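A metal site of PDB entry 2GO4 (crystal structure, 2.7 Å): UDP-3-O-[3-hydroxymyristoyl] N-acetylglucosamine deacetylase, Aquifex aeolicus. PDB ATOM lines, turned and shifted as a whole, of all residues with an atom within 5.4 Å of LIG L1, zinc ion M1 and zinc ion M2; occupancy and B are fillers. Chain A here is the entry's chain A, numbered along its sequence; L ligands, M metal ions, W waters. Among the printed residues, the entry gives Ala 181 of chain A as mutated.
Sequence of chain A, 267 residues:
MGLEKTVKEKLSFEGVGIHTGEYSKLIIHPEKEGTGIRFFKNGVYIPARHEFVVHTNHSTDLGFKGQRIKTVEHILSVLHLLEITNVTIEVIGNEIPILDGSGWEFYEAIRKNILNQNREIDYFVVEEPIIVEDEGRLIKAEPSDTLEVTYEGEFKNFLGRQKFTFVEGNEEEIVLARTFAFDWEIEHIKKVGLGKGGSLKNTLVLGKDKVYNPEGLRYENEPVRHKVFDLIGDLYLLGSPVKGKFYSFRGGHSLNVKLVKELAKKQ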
ATOM      1  N   ILE A  18      16.632  20.608  28.739  1.00  0.00           N
ATOM      2  CA  ILE A  18      15.623  19.557  28.796  1.00  0.00           C
ATOM      3  C   ILE A  18      15.675  18.652  30.036  1.00  0.00           C
ATOM      4  O   ILE A  18      14.644  18.139  30.478  1.00  0.00           O
ATOM      5  CB  ILE A  18      15.666  18.681  27.509  1.00  0.00           C
ATOM      6  CG1 ILE A  18      14.398  17.829  27.453  1.00  0.00           C
ATOM      7  CG2 ILE A  18      16.936  17.801  27.485  1.00  0.00           C
ATOM      8  CD1 ILE A  18      14.130  17.205  26.097  1.00  0.00           C
ATOM      9  N   HIS A  19      16.846  18.462  30.617  1.00  0.00           N
ATOM     10  CA  HIS A  19      16.938  17.601  31.783  1.00  0.00           C
ATOM     11  C   HIS A  19      16.907  18.316  33.127  1.00  0.00           C
ATOM     12  O   HIS A  19      16.253  17.861  34.060  1.00  0.00           O
ATOM     13  CB  HIS A  19      18.182  16.722  31.705  1.00  0.00           C
ATOM     14  CG  HIS A  19      18.115  15.664  30.655  1.00  0.00           C
ATOM     15  ND1 HIS A  19      17.040  14.800  30.541  1.00  0.00           N
ATOM     16  CD2 HIS A  19      18.985  15.299  29.686  1.00  0.00           C
ATOM     17  CE1 HIS A  19      17.260  13.954  29.550  1.00  0.00           C
ATOM     18  NE2 HIS A  19      18.431  14.232  29.011  1.00  0.00           N
ATOM     19  N   ASN A  57      23.533   8.564  29.653  1.00  0.00           N
ATOM     20  CA  ASN A  57      22.159   8.100  29.750  1.00  0.00           C
ATOM     21  C   ASN A  57      21.223   9.260  29.440  1.00  0.00           C
ATOM     22  O   ASN A  57      21.178  10.241  30.183  1.00  0.00           O
ATOM     23  CB  ASN A  57      21.836   7.594  31.160  1.00  0.00           C
ATOM     24  CG  ASN A  57      22.672   6.397  31.561  1.00  0.00           C
ATOM     25  OD1 ASN A  57      22.569   5.928  32.690  1.00  0.00           O
ATOM     26  ND2 ASN A  57      23.497   5.906  30.630  1.00  0.00           N
ATOM     27  N   HIS A  58      20.480   9.155  28.344  1.00  0.00           N
ATOM     28  CA  HIS A  58      19.528  10.197  27.962  1.00  0.00           C
ATOM     29  C   HIS A  58      20.158  11.480  27.457  1.00  0.00           C
ATOM     30  O   HIS A  58      19.459  12.426  27.116  1.00  0.00           O
ATOM     31  CB  HIS A  58      18.601  10.509  29.141  1.00  0.00           C
ATOM     32  CG  HIS A  58      17.922   9.293  29.692  1.00  0.00           C
ATOM     33  ND1 HIS A  58      16.995   8.569  28.960  1.00  0.00           N
ATOM     34  CD2 HIS A  58      18.075   8.644  30.866  1.00  0.00           C
ATOM     35  CE1 HIS A  58      16.621   7.514  29.665  1.00  0.00           C
ATOM     36  NE2 HIS A  58      17.257   7.537  30.824  1.00  0.00           N
ATOM     37  N   SER A  59      21.483  11.510  27.420  1.00  0.00           N
ATOM     38  CA  SER A  59      22.202  12.682  26.934  1.00  0.00           C
ATOM     39  C   SER A  59      23.666  12.429  27.113  1.00  0.00           C
ATOM     40  O   SER A  59      24.053  11.494  27.794  1.00  0.00           O
ATOM     41  CB  SER A  59      21.830  13.941  27.715  1.00  0.00           C
ATOM     42  OG  SER A  59      22.396  13.963  29.015  1.00  0.00           O
ATOM     43  N   GLU A  73      25.556  17.129  22.947  1.00  0.00           N
ATOM     44  CA  GLU A  73      25.382  16.501  21.638  1.00  0.00           C
ATOM     45  C   GLU A  73      24.727  17.297  20.525  1.00  0.00           C
ATOM     46  O   GLU A  73      25.179  17.224  19.383  1.00  0.00           O
ATOM     47  CB  GLU A  73      24.649  15.165  21.804  1.00  0.00           C
ATOM     48  CG  GLU A  73      23.223  15.314  22.287  1.00  0.00           C
ATOM     49  CD  GLU A  73      23.060  14.962  23.745  1.00  0.00           C
ATOM     50  OE1 GLU A  73      24.021  15.162  24.525  1.00  0.00           O
ATOM     51  OE2 GLU A  73      21.958  14.488  24.112  1.00  0.00           O
ATOM     52  N   HIS A  74      23.684  18.050  20.796  1.00  0.00           N
ATOM     53  CA  HIS A  74      23.035  18.772  19.719  1.00  0.00           C
ATOM     54  C   HIS A  74      23.867  19.944  19.160  1.00  0.00           C
ATOM     55  O   HIS A  74      23.931  20.161  17.953  1.00  0.00           O
ATOM     56  CB  HIS A  74      21.649  19.238  20.148  1.00  0.00           C
ATOM     57  CG  HIS A  74      20.739  18.103  20.515  1.00  0.00           C
ATOM     58  ND1 HIS A  74      19.426  18.299  20.912  1.00  0.00           N
ATOM     59  CD2 HIS A  74      20.948  16.774  20.565  1.00  0.00           C
ATOM     60  CE1 HIS A  74      18.882  17.130  21.183  1.00  0.00           C
ATOM     61  NE2 HIS A  74      19.776  16.186  20.985  1.00  0.00           N
ATOM     62  N   GLY A 101      14.415  21.212  20.514  1.00  0.00           N
ATOM     63  CA  GLY A 101      14.699  19.789  20.542  1.00  0.00           C
ATOM     64  C   GLY A 101      15.563  19.297  19.393  1.00  0.00           C
ATOM     65  O   GLY A 101      16.052  18.161  19.440  1.00  0.00           O
ATOM     66  N   THR A 179      14.202  15.834  19.386  1.00  0.00           N
ATOM     67  CA  THR A 179      14.387  14.830  20.428  1.00  0.00           C
ATOM     68  C   THR A 179      13.035  14.150  20.629  1.00  0.00           C
ATOM     69  O   THR A 179      11.988  14.804  20.683  1.00  0.00           O
ATOM     70  CB  THR A 179      14.784  15.497  21.742  1.00  0.00           C
ATOM     71  OG1 THR A 179      16.037  16.149  21.573  1.00  0.00           O
ATOM     72  CG2 THR A 179      14.864  14.490  22.860  1.00  0.00           C
ATOM     73  N   PHE A 180      13.049  12.834  20.776  1.00  0.00           N
ATOM     74  CA  PHE A 180      11.793  12.128  20.964  1.00  0.00           C
ATOM     75  C   PHE A 180      11.889  11.160  22.141  1.00  0.00           C
ATOM     76  O   PHE A 180      12.970  10.700  22.513  1.00  0.00           O
ATOM     77  CB  PHE A 180      11.461  11.362  19.683  1.00  0.00           C
ATOM     78  CG  PHE A 180      12.369  10.213  19.436  1.00  0.00           C
ATOM     79  CD1 PHE A 180      12.086   8.952  19.953  1.00  0.00           C
ATOM     80  CD2 PHE A 180      13.564  10.405  18.736  1.00  0.00           C
ATOM     81  CE1 PHE A 180      12.966   7.896  19.782  1.00  0.00           C
ATOM     82  CE2 PHE A 180      14.462   9.360  18.557  1.00  0.00           C
ATOM     83  CZ  PHE A 180      14.165   8.101  19.085  1.00  0.00           C
ATOM     84  N   ALA A 181      10.737  10.841  22.715  1.00  0.00           N
ATOM     85  CA  ALA A 181      10.663   9.903  23.833  1.00  0.00           C
ATOM     86  C   ALA A 181       9.313   9.219  23.763  1.00  0.00           C
ATOM     87  O   ALA A 181       8.364   9.747  23.171  1.00  0.00           O
ATOM     88  CB  ALA A 181      10.825  10.620  25.171  1.00  0.00           C
ATOM     89  N   ASP A 183       5.967   7.608  25.697  1.00  0.00           N
ATOM     90  CA  ASP A 183       5.207   7.864  26.918  1.00  0.00           C
ATOM     91  C   ASP A 183       5.621   6.935  28.052  1.00  0.00           C
ATOM     92  O   ASP A 183       5.653   7.344  29.225  1.00  0.00           O
ATOM     93  CB  ASP A 183       3.694   7.778  26.667  1.00  0.00           C
ATOM     94  CG  ASP A 183       3.291   6.550  25.873  1.00  0.00           C
ATOM     95  OD1 ASP A 183       4.031   5.554  25.881  1.00  0.00           O
ATOM     96  OD2 ASP A 183       2.207   6.577  25.263  1.00  0.00           O
ATOM     97  N   GLU A 185       8.574   5.740  28.674  1.00  0.00           N
ATOM     98  CA  GLU A 185       9.897   6.135  29.179  1.00  0.00           C
ATOM     99  C   GLU A 185       9.806   7.247  30.228  1.00  0.00           C
ATOM    100  O   GLU A 185      10.531   7.244  31.230  1.00  0.00           O
ATOM    101  CB  GLU A 185      10.754   6.686  28.045  1.00  0.00           C
ATOM    102  CG  GLU A 185      11.406   5.719  27.099  1.00  0.00           C
ATOM    103  CD  GLU A 185      12.457   6.438  26.252  1.00  0.00           C
ATOM    104  OE1 GLU A 185      12.093   7.375  25.504  1.00  0.00           O
ATOM    105  OE2 GLU A 185      13.657   6.088  26.355  1.00  0.00           O
ATOM    106  N   ILE A 186       8.925   8.197  29.965  1.00  0.00           N
ATOM    107  CA  ILE A 186       8.738   9.371  30.801  1.00  0.00           C
ATOM    108  C   ILE A 186       8.728   9.202  32.323  1.00  0.00           C
ATOM    109  O   ILE A 186       9.464   9.897  33.031  1.00  0.00           O
ATOM    110  CB  ILE A 186       7.470  10.114  30.353  1.00  0.00           C
ATOM    111  CG1 ILE A 186       7.622  10.529  28.894  1.00  0.00           C
ATOM    112  CG2 ILE A 186       7.235  11.347  31.228  1.00  0.00           C
ATOM    113  CD1 ILE A 186       6.434  11.252  28.323  1.00  0.00           C
ATOM    114  N   HIS A 188       9.968   7.006  34.046  1.00  0.00           N
ATOM    115  CA  HIS A 188      11.298   6.598  34.427  1.00  0.00           C
ATOM    116  C   HIS A 188      12.262   7.763  34.389  1.00  0.00           C
ATOM    117  O   HIS A 188      12.994   8.019  35.345  1.00  0.00           O
ATOM    118  CB  HIS A 188      11.806   5.533  33.477  1.00  0.00           C
ATOM    119  CG  HIS A 188      13.300   5.466  33.398  1.00  0.00           C
ATOM    120  ND1 HIS A 188      14.072   4.983  34.425  1.00  0.00           N
ATOM    121  CD2 HIS A 188      14.155   5.845  32.420  1.00  0.00           C
ATOM    122  CE1 HIS A 188      15.352   5.072  34.089  1.00  0.00           C
ATOM    123  NE2 HIS A 188      15.424   5.593  32.876  1.00  0.00           N
ATOM    124  N   ILE A 189      12.267   8.475  33.274  1.00  0.00           N
ATOM    125  CA  ILE A 189      13.150   9.621  33.130  1.00  0.00           C
ATOM    126  C   ILE A 189      12.896  10.606  34.264  1.00  0.00           C
ATOM    127  O   ILE A 189      13.832  11.142  34.841  1.00  0.00           O
ATOM    128  CB  ILE A 189      12.947  10.315  31.759  1.00  0.00           C
ATOM    129  CG1 ILE A 189      13.467   9.389  30.655  1.00  0.00           C
ATOM    130  CG2 ILE A 189      13.678  11.639  31.721  1.00  0.00           C
ATOM    131  CD1 ILE A 189      13.163   9.877  29.269  1.00  0.00           C
ATOM    132  N   LYS A 190      11.619  10.825  34.578  1.00  0.00           N
ATOM    133  CA  LYS A 190      11.279  11.744  35.671  1.00  0.00           C
ATOM    134  C   LYS A 190      11.786  11.225  37.016  1.00  0.00           C
ATOM    135  O   LYS A 190      12.261  12.001  37.852  1.00  0.00           O
ATOM    136  CB  LYS A 190       9.771  11.962  35.715  1.00  0.00           C
ATOM    137  CG  LYS A 190       9.240  12.901  34.644  1.00  0.00           C
ATOM    138  CD  LYS A 190       9.647  14.330  34.946  1.00  0.00           C
ATOM    139  CE  LYS A 190       8.945  15.312  34.027  1.00  0.00           C
ATOM    140  NZ  LYS A 190       9.152  16.714  34.496  1.00  0.00           N
ATOM    141  N   VAL A 192      14.449   9.270  37.710  1.00  0.00           N
ATOM    142  CA  VAL A 192      15.903   9.355  37.842  1.00  0.00           C
ATOM    143  C   VAL A 192      16.460  10.779  37.828  1.00  0.00           C
ATOM    144  O   VAL A 192      17.665  10.972  37.688  1.00  0.00           O
ATOM    145  CB  VAL A 192      16.598   8.542  36.730  1.00  0.00           C
ATOM    146  CG1 VAL A 192      16.170   7.089  36.826  1.00  0.00           C
ATOM    147  CG2 VAL A 192      16.238   9.103  35.357  1.00  0.00           C
ATOM    148  N   LEU A 194      15.677  13.317  35.607  1.00  0.00           N
ATOM    149  CA  LEU A 194      15.890  13.936  34.306  1.00  0.00           C
ATOM    150  C   LEU A 194      14.609  14.503  33.717  1.00  0.00           C
ATOM    151  O   LEU A 194      13.597  14.596  34.398  1.00  0.00           O
ATOM    152  CB  LEU A 194      16.531  12.912  33.368  1.00  0.00           C
ATOM    153  CG  LEU A 194      17.846  12.321  33.900  1.00  0.00           C
ATOM    154  CD1 LEU A 194      18.402  11.322  32.910  1.00  0.00           C
ATOM    155  CD2 LEU A 194      18.847  13.442  34.135  1.00  0.00           C
ATOM    156  N   GLY A 195      14.681  14.912  32.454  1.00  0.00           N
ATOM    157  CA  GLY A 195      13.528  15.457  31.760  1.00  0.00           C
ATOM    158  C   GLY A 195      12.755  16.555  32.475  1.00  0.00           C
ATOM    159  O   GLY A 195      11.608  16.832  32.108  1.00  0.00           O
ATOM    160  N   GLY A 198      11.428  19.047  30.005  1.00  0.00           N
ATOM    161  CA  GLY A 198      10.805  18.553  28.783  1.00  0.00           C
ATOM    162  C   GLY A 198       9.327  18.822  28.629  1.00  0.00           C
ATOM    163  O   GLY A 198       8.534  18.650  29.540  1.00  0.00           O
ATOM    164  N   SER A 199       8.945  19.237  27.430  1.00  0.00           N
ATOM    165  CA  SER A 199       7.542  19.513  27.130  1.00  0.00           C
ATOM    166  C   SER A 199       7.278  19.085  25.701  1.00  0.00           C
ATOM    167  O   SER A 199       8.153  18.506  25.055  1.00  0.00           O
ATOM    168  CB  SER A 199       7.260  21.003  27.293  1.00  0.00           C
ATOM    169  OG  SER A 199       7.964  21.754  26.324  1.00  0.00           O
ATOM    170  N   LEU A 200       6.081  19.345  25.203  1.00  0.00           N
ATOM    171  CA  LEU A 200       5.774  18.981  23.837  1.00  0.00           C
ATOM    172  C   LEU A 200       6.368  20.033  22.910  1.00  0.00           C
ATOM    173  O   LEU A 200       6.286  19.915  21.689  1.00  0.00           O
ATOM    174  CB  LEU A 200       4.259  18.896  23.624  1.00  0.00           C
ATOM    175  CG  LEU A 200       3.523  17.797  24.400  1.00  0.00           C
ATOM    176  CD1 LEU A 200       2.070  17.770  23.934  1.00  0.00           C
ATOM    177  CD2 LEU A 200       4.163  16.442  24.168  1.00  0.00           C
ATOM    178  N   THR A 203      10.170  18.264  22.802  1.00  0.00           N
ATOM    179  CA  THR A 203      10.247  16.808  22.718  1.00  0.00           C
ATOM    180  C   THR A 203       9.075  16.265  21.914  1.00  0.00           C
ATOM    181  O   THR A 203       7.964  16.779  21.977  1.00  0.00           O
ATOM    182  CB  THR A 203      10.198  16.167  24.136  1.00  0.00           C
ATOM    183  OG1 THR A 203      11.183  16.789  24.982  1.00  0.00           O
ATOM    184  CG2 THR A 203      10.469  14.661  24.050  1.00  0.00           C
ATOM    185  N   VAL A 205       6.697  13.323  21.734  1.00  0.00           N
ATOM    186  CA  VAL A 205       6.261  12.171  22.518  1.00  0.00           C
ATOM    187  C   VAL A 205       5.448  11.203  21.695  1.00  0.00           C
ATOM    188  O   VAL A 205       4.484  11.571  21.014  1.00  0.00           O
ATOM    189  CB  VAL A 205       5.463  12.605  23.771  1.00  0.00           C
ATOM    190  CG1 VAL A 205       5.325  11.420  24.727  1.00  0.00           C
ATOM    191  CG2 VAL A 205       6.161  13.777  24.457  1.00  0.00           C
ATOM    192  N   TYR A 212       1.612  12.265  20.488  1.00  0.00           N
ATOM    193  CA  TYR A 212       1.009  13.267  21.356  1.00  0.00           C
ATOM    194  C   TYR A 212       1.104  14.670  20.816  1.00  0.00           C
ATOM    195  O   TYR A 212       0.150  15.428  20.932  1.00  0.00           O
ATOM    196  CB  TYR A 212       1.643  13.218  22.745  1.00  0.00           C
ATOM    197  CG  TYR A 212       1.305  11.972  23.506  1.00  0.00           C
ATOM    198  CD1 TYR A 212       1.964  10.772  23.250  1.00  0.00           C
ATOM    199  CD2 TYR A 212       0.325  11.985  24.503  1.00  0.00           C
ATOM    200  CE1 TYR A 212       1.656   9.616  23.951  1.00  0.00           C
ATOM    201  CE2 TYR A 212       0.012  10.829  25.217  1.00  0.00           C
ATOM    202  CZ  TYR A 212       0.679   9.660  24.935  1.00  0.00           C
ATOM    203  OH  TYR A 212       0.398   8.519  25.639  1.00  0.00           O
ATOM    204  N   HIS A 226      16.921  11.800  13.933  1.00  0.00           N
ATOM    205  CA  HIS A 226      17.469  12.432  15.127  1.00  0.00           C
ATOM    206  C   HIS A 226      18.571  11.588  15.730  1.00  0.00           C
ATOM    207  O   HIS A 226      19.531  12.105  16.284  1.00  0.00           O
ATOM    208  CB  HIS A 226      16.395  12.673  16.176  1.00  0.00           C
ATOM    209  CG  HIS A 226      16.899  13.431  17.367  1.00  0.00           C
ATOM    210  ND1 HIS A 226      17.069  14.799  17.355  1.00  0.00           N
ATOM    211  CD2 HIS A 226      17.366  12.999  18.558  1.00  0.00           C
ATOM    212  CE1 HIS A 226      17.627  15.176  18.489  1.00  0.00           C
ATOM    213  NE2 HIS A 226      17.811  14.112  19.242  1.00  0.00           N
ATOM    214  N   LYS A 227      18.425  10.275  15.632  1.00  0.00           N
ATOM    215  CA  LYS A 227      19.450   9.384  16.152  1.00  0.00           C
ATOM    216  C   LYS A 227      20.733   9.565  15.348  1.00  0.00           C
ATOM    217  O   LYS A 227      21.830   9.441  15.884  1.00  0.00           O
ATOM    218  CB  LYS A 227      18.957   7.951  16.098  1.00  0.00           C
ATOM    219  CG  LYS A 227      17.978   7.613  17.191  1.00  0.00           C
ATOM    220  CD  LYS A 227      18.689   7.439  18.518  1.00  0.00           C
ATOM    221  CE  LYS A 227      17.705   7.333  19.665  1.00  0.00           C
ATOM    222  NZ  LYS A 227      18.416   7.047  20.943  1.00  0.00           N
ATOM    223  N   PHE A 229      21.534  12.416  13.856  1.00  0.00           N
ATOM    224  CA  PHE A 229      21.964  13.712  14.347  1.00  0.00           C
ATOM    225  C   PHE A 229      22.715  13.538  15.689  1.00  0.00           C
ATOM    226  O   PHE A 229      23.759  14.151  15.894  1.00  0.00           O
ATOM    227  CB  PHE A 229      20.735  14.598  14.551  1.00  0.00           C
ATOM    228  CG  PHE A 229      21.041  15.972  15.061  1.00  0.00           C
ATOM    229  CD1 PHE A 229      21.582  16.954  14.217  1.00  0.00           C
ATOM    230  CD2 PHE A 229      20.759  16.319  16.374  1.00  0.00           C
ATOM    231  CE1 PHE A 229      21.828  18.248  14.688  1.00  0.00           C
ATOM    232  CE2 PHE A 229      21.001  17.612  16.858  1.00  0.00           C
ATOM    233  CZ  PHE A 229      21.542  18.587  16.007  1.00  0.00           C
ATOM    234  N   ASP A 230      22.185  12.709  16.589  1.00  0.00           N
ATOM    235  CA  ASP A 230      22.858  12.508  17.872  1.00  0.00           C
ATOM    236  C   ASP A 230      24.217  11.856  17.688  1.00  0.00           C
ATOM    237  O   ASP A 230      25.175  12.258  18.326  1.00  0.00           O
ATOM    238  CB  ASP A 230      22.052  11.611  18.828  1.00  0.00           C
ATOM    239  CG  ASP A 230      20.903  12.333  19.511  1.00  0.00           C
ATOM    240  OD1 ASP A 230      20.975  13.567  19.684  1.00  0.00           O
ATOM    241  OD2 ASP A 230      19.942  11.649  19.903  1.00  0.00           O
ATOM    242  N   HIS A 253      23.780   6.998  22.944  1.00  0.00           N
ATOM    243  CA  HIS A 253      24.940   7.735  23.429  1.00  0.00           C
ATOM    244  C   HIS A 253      26.022   6.843  24.044  1.00  0.00           C
ATOM    245  O   HIS A 253      27.194   6.952  23.686  1.00  0.00           O
ATOM    246  CB  HIS A 253      24.503   8.800  24.434  1.00  0.00           C
ATOM    247  CG  HIS A 253      23.599   9.834  23.866  1.00  0.00           C
ATOM    248  ND1 HIS A 253      23.966  10.653  22.810  1.00  0.00           N
ATOM    249  CD2 HIS A 253      22.348  10.220  24.212  1.00  0.00           C
ATOM    250  CE1 HIS A 253      22.982  11.486  22.535  1.00  0.00           C
ATOM    251  NE2 HIS A 253      21.983  11.247  23.363  1.00  0.00           N
HETATM  252  C1  LIG L   1      16.213  10.630  25.364  1.00  0.00           C
HETATM  253  C2  LIG L   1      15.849   9.153  25.249  1.00  0.00           C
HETATM  254  C3  LIG L   1      17.125   8.301  25.267  1.00  0.00           C
HETATM  255  C4  LIG L   1      17.174  11.008  24.237  1.00  0.00           C
HETATM  256  C5  LIG L   1      18.387  10.064  24.250  1.00  0.00           C
HETATM  257  O1  LIG L   1      17.951   8.694  24.159  1.00  0.00           O
HETATM  258  O2  LIG L   1      15.030  11.431  25.250  1.00  0.00           O
HETATM  259  O3  LIG L   1      15.546  12.186  27.317  1.00  0.00           O
HETATM  260  C6  LIG L   1      14.805  12.228  26.334  1.00  0.00           C
HETATM  261  C7  LIG L   1      13.576  13.141  26.306  1.00  0.00           C
HETATM  262  C8  LIG L   1      13.245  13.724  27.680  1.00  0.00           C
HETATM  263  C9  LIG L   1      11.727  13.960  27.773  1.00  0.00           C
HETATM  264  C10 LIG L   1      11.330  14.663  29.069  1.00  0.00           C
HETATM  265  C11 LIG L   1       9.862  14.441  29.429  1.00  0.00           C
HETATM  266  C12 LIG L   1       8.873  14.885  28.346  1.00  0.00           C
HETATM  267  C13 LIG L   1       7.450  14.778  28.885  1.00  0.00           C
HETATM  268  C14 LIG L   1       6.393  15.082  27.824  1.00  0.00           C
HETATM  269  C15 LIG L   1       5.003  15.166  28.466  1.00  0.00           C
HETATM  270  C16 LIG L   1       3.890  15.377  27.440  1.00  0.00           C
HETATM  271  C17 LIG L   1       3.456  14.085  26.738  1.00  0.00           C
HETATM  272  C18 LIG L   1       2.540  13.197  27.603  1.00  0.00           C
HETATM  273  C19 LIG L   1       3.264  12.583  28.802  1.00  0.00           C
HETATM  274  C20 LIG L   1      17.601  12.469  24.381  1.00  0.00           C
HETATM  275  C21 LIG L   1      18.304  13.009  23.131  1.00  0.00           C
HETATM  276  O4  LIG L   1      17.653  13.430  22.175  1.00  0.00           O
HETATM  277  N1  LIG L   1      19.634  12.973  23.176  1.00  0.00           N
HETATM  278  O5  LIG L   1      20.343  13.473  22.129  1.00  0.00           O
HETATM  279  O6  LIG L   1      15.013   8.787  26.347  1.00  0.00           O
HETATM  280  C22 LIG L   1      16.756   6.824  25.165  1.00  0.00           C
HETATM  281  O7  LIG L   1      17.916   6.013  25.338  1.00  0.00           O
HETATM  282 CL1  LG2 L   2      18.031   4.550  31.308  1.00  0.00          CL
HETATM  283 ZN    ZN M   1      19.181  14.202  20.734  1.00  0.00          ZN
HETATM  284 ZN    ZN M   2      17.622   6.139  32.438  1.00  0.00          ZN
HETATM  285  O   HOH W   1      19.116   6.750  34.036  1.00  0.00           O
HETATM  286  O   HOH W   2      20.585   7.470  25.493  1.00  0.00           O
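Water W2 bridges O7 of LIG L1 and N of His 58.
Ile 18 touches LIG L1 (CD1 to C8, 3.9 Å). His 19 touches LIG L1 (CE1 to O3, 3.3 Å). Phe 180 touches LIG L1. CB of Ala 181 touches C7 of LIG L1 (3.9 Å). Ile 186 touches LIG L1 (CD1 to C19, 3.5 Å). Ile 189 touches LIG L1. Gly 195 touches LIG L1 (CA to C10, 3.6 Å). Gly 198 touches LIG L1. Leu 200 touches LIG L1. Thr 203 touches LIG L1. Val 205 touches LIG L1. Tyr 212 touches LIG L1 (CD2 to C18, 3.998 Å). NZ of Lys 227 touches O1 of LIG L1, at 3.6 Å. Hydrophobic or aromatic side chains within 4 Å of LIG L1: Ile 18, His 19, His 58, His 74, Ala 181, Ile 186, Ile 189, Leu 200, Val 205, Tyr 212, His 226 and His 253. Along chain A the residues within 4 Å of LIG L1 span positions 18 to 253.
The backbone carbonyl oxygen (O) of Val 205 is in hydrogen-bond range of the backbone NH (N) of Tyr 212, 3.0 Å away. ND1 of His 19 sits at hydrogen-bond distance from N of Gly 195 (3.0 Å). O of Ile 189 sits at hydrogen-bond distance from N of Leu 194. O of Gly 195 is in hydrogen-bond range of NZ of Lys 190 (3.4 Å). OE2 of Glu 73 sits at hydrogen-bond distance from NE2 of His 253. The side-chain hydroxyl of Tyr 212 is in hydrogen-bond range of the side-chain carboxylate of Asp 183 (2.7 Å). OG1 of Thr 203 sits close to O of Ser 199 (3.5 Å). O of Ile 18 lies within hydrogen-bond range of N of Gly 198.
Thr 179 touches zinc ion M1. Within 4 Å of zinc ion M1: His 74, Thr 179, His 226 and Asp 230.
The nearest printed residue that does not touch zinc ion M2 is Val 192 (4.4 Å).
O5 of LIG L1 binds zinc ion M1. Zinc ion M1 is bound by NE2 of His 226 (2.0 Å). Zinc ion M1 is bound by NE2 of His 74. OD1 of Asp 230 binds zinc ion M1 (2.2 Å). Zinc ion M1 is bound by O4 of LIG L1, 2.2 Å away. Zinc ion M1 has five donor atoms within binding distance. Slightly farther from zinc ion M1 lies the side-chain carboxylate (OD2) of Asp 230 (2.8 Å).
N1 of LIG L1 sits at hydrogen-bond distance from NE2 of His 253, 2.9 Å away. The side-chain hydroxyl of Thr 179 sits close to an oxygen (O4) of LIG L1, at 3.2 Å. The side-chain carboxylate of Glu 73 is in hydrogen-bond range of a nitrogen (N1) of LIG L1. A ring nitrogen (ND1) of His 58 is in hydrogen-bond range of an oxygen (O6) of LIG L1 (3.3 Å). OE2 of Glu 185 lies within hydrogen-bond range of O6 of LIG L1 (3.0 Å).
Zinc ion M2 is bound by CL1 of LG2 L2 (2.0 Å), NE2 of His 58 (2.2 Å), water W1 (2.3 Å) and NE2 of His 188 (2.3 Å).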
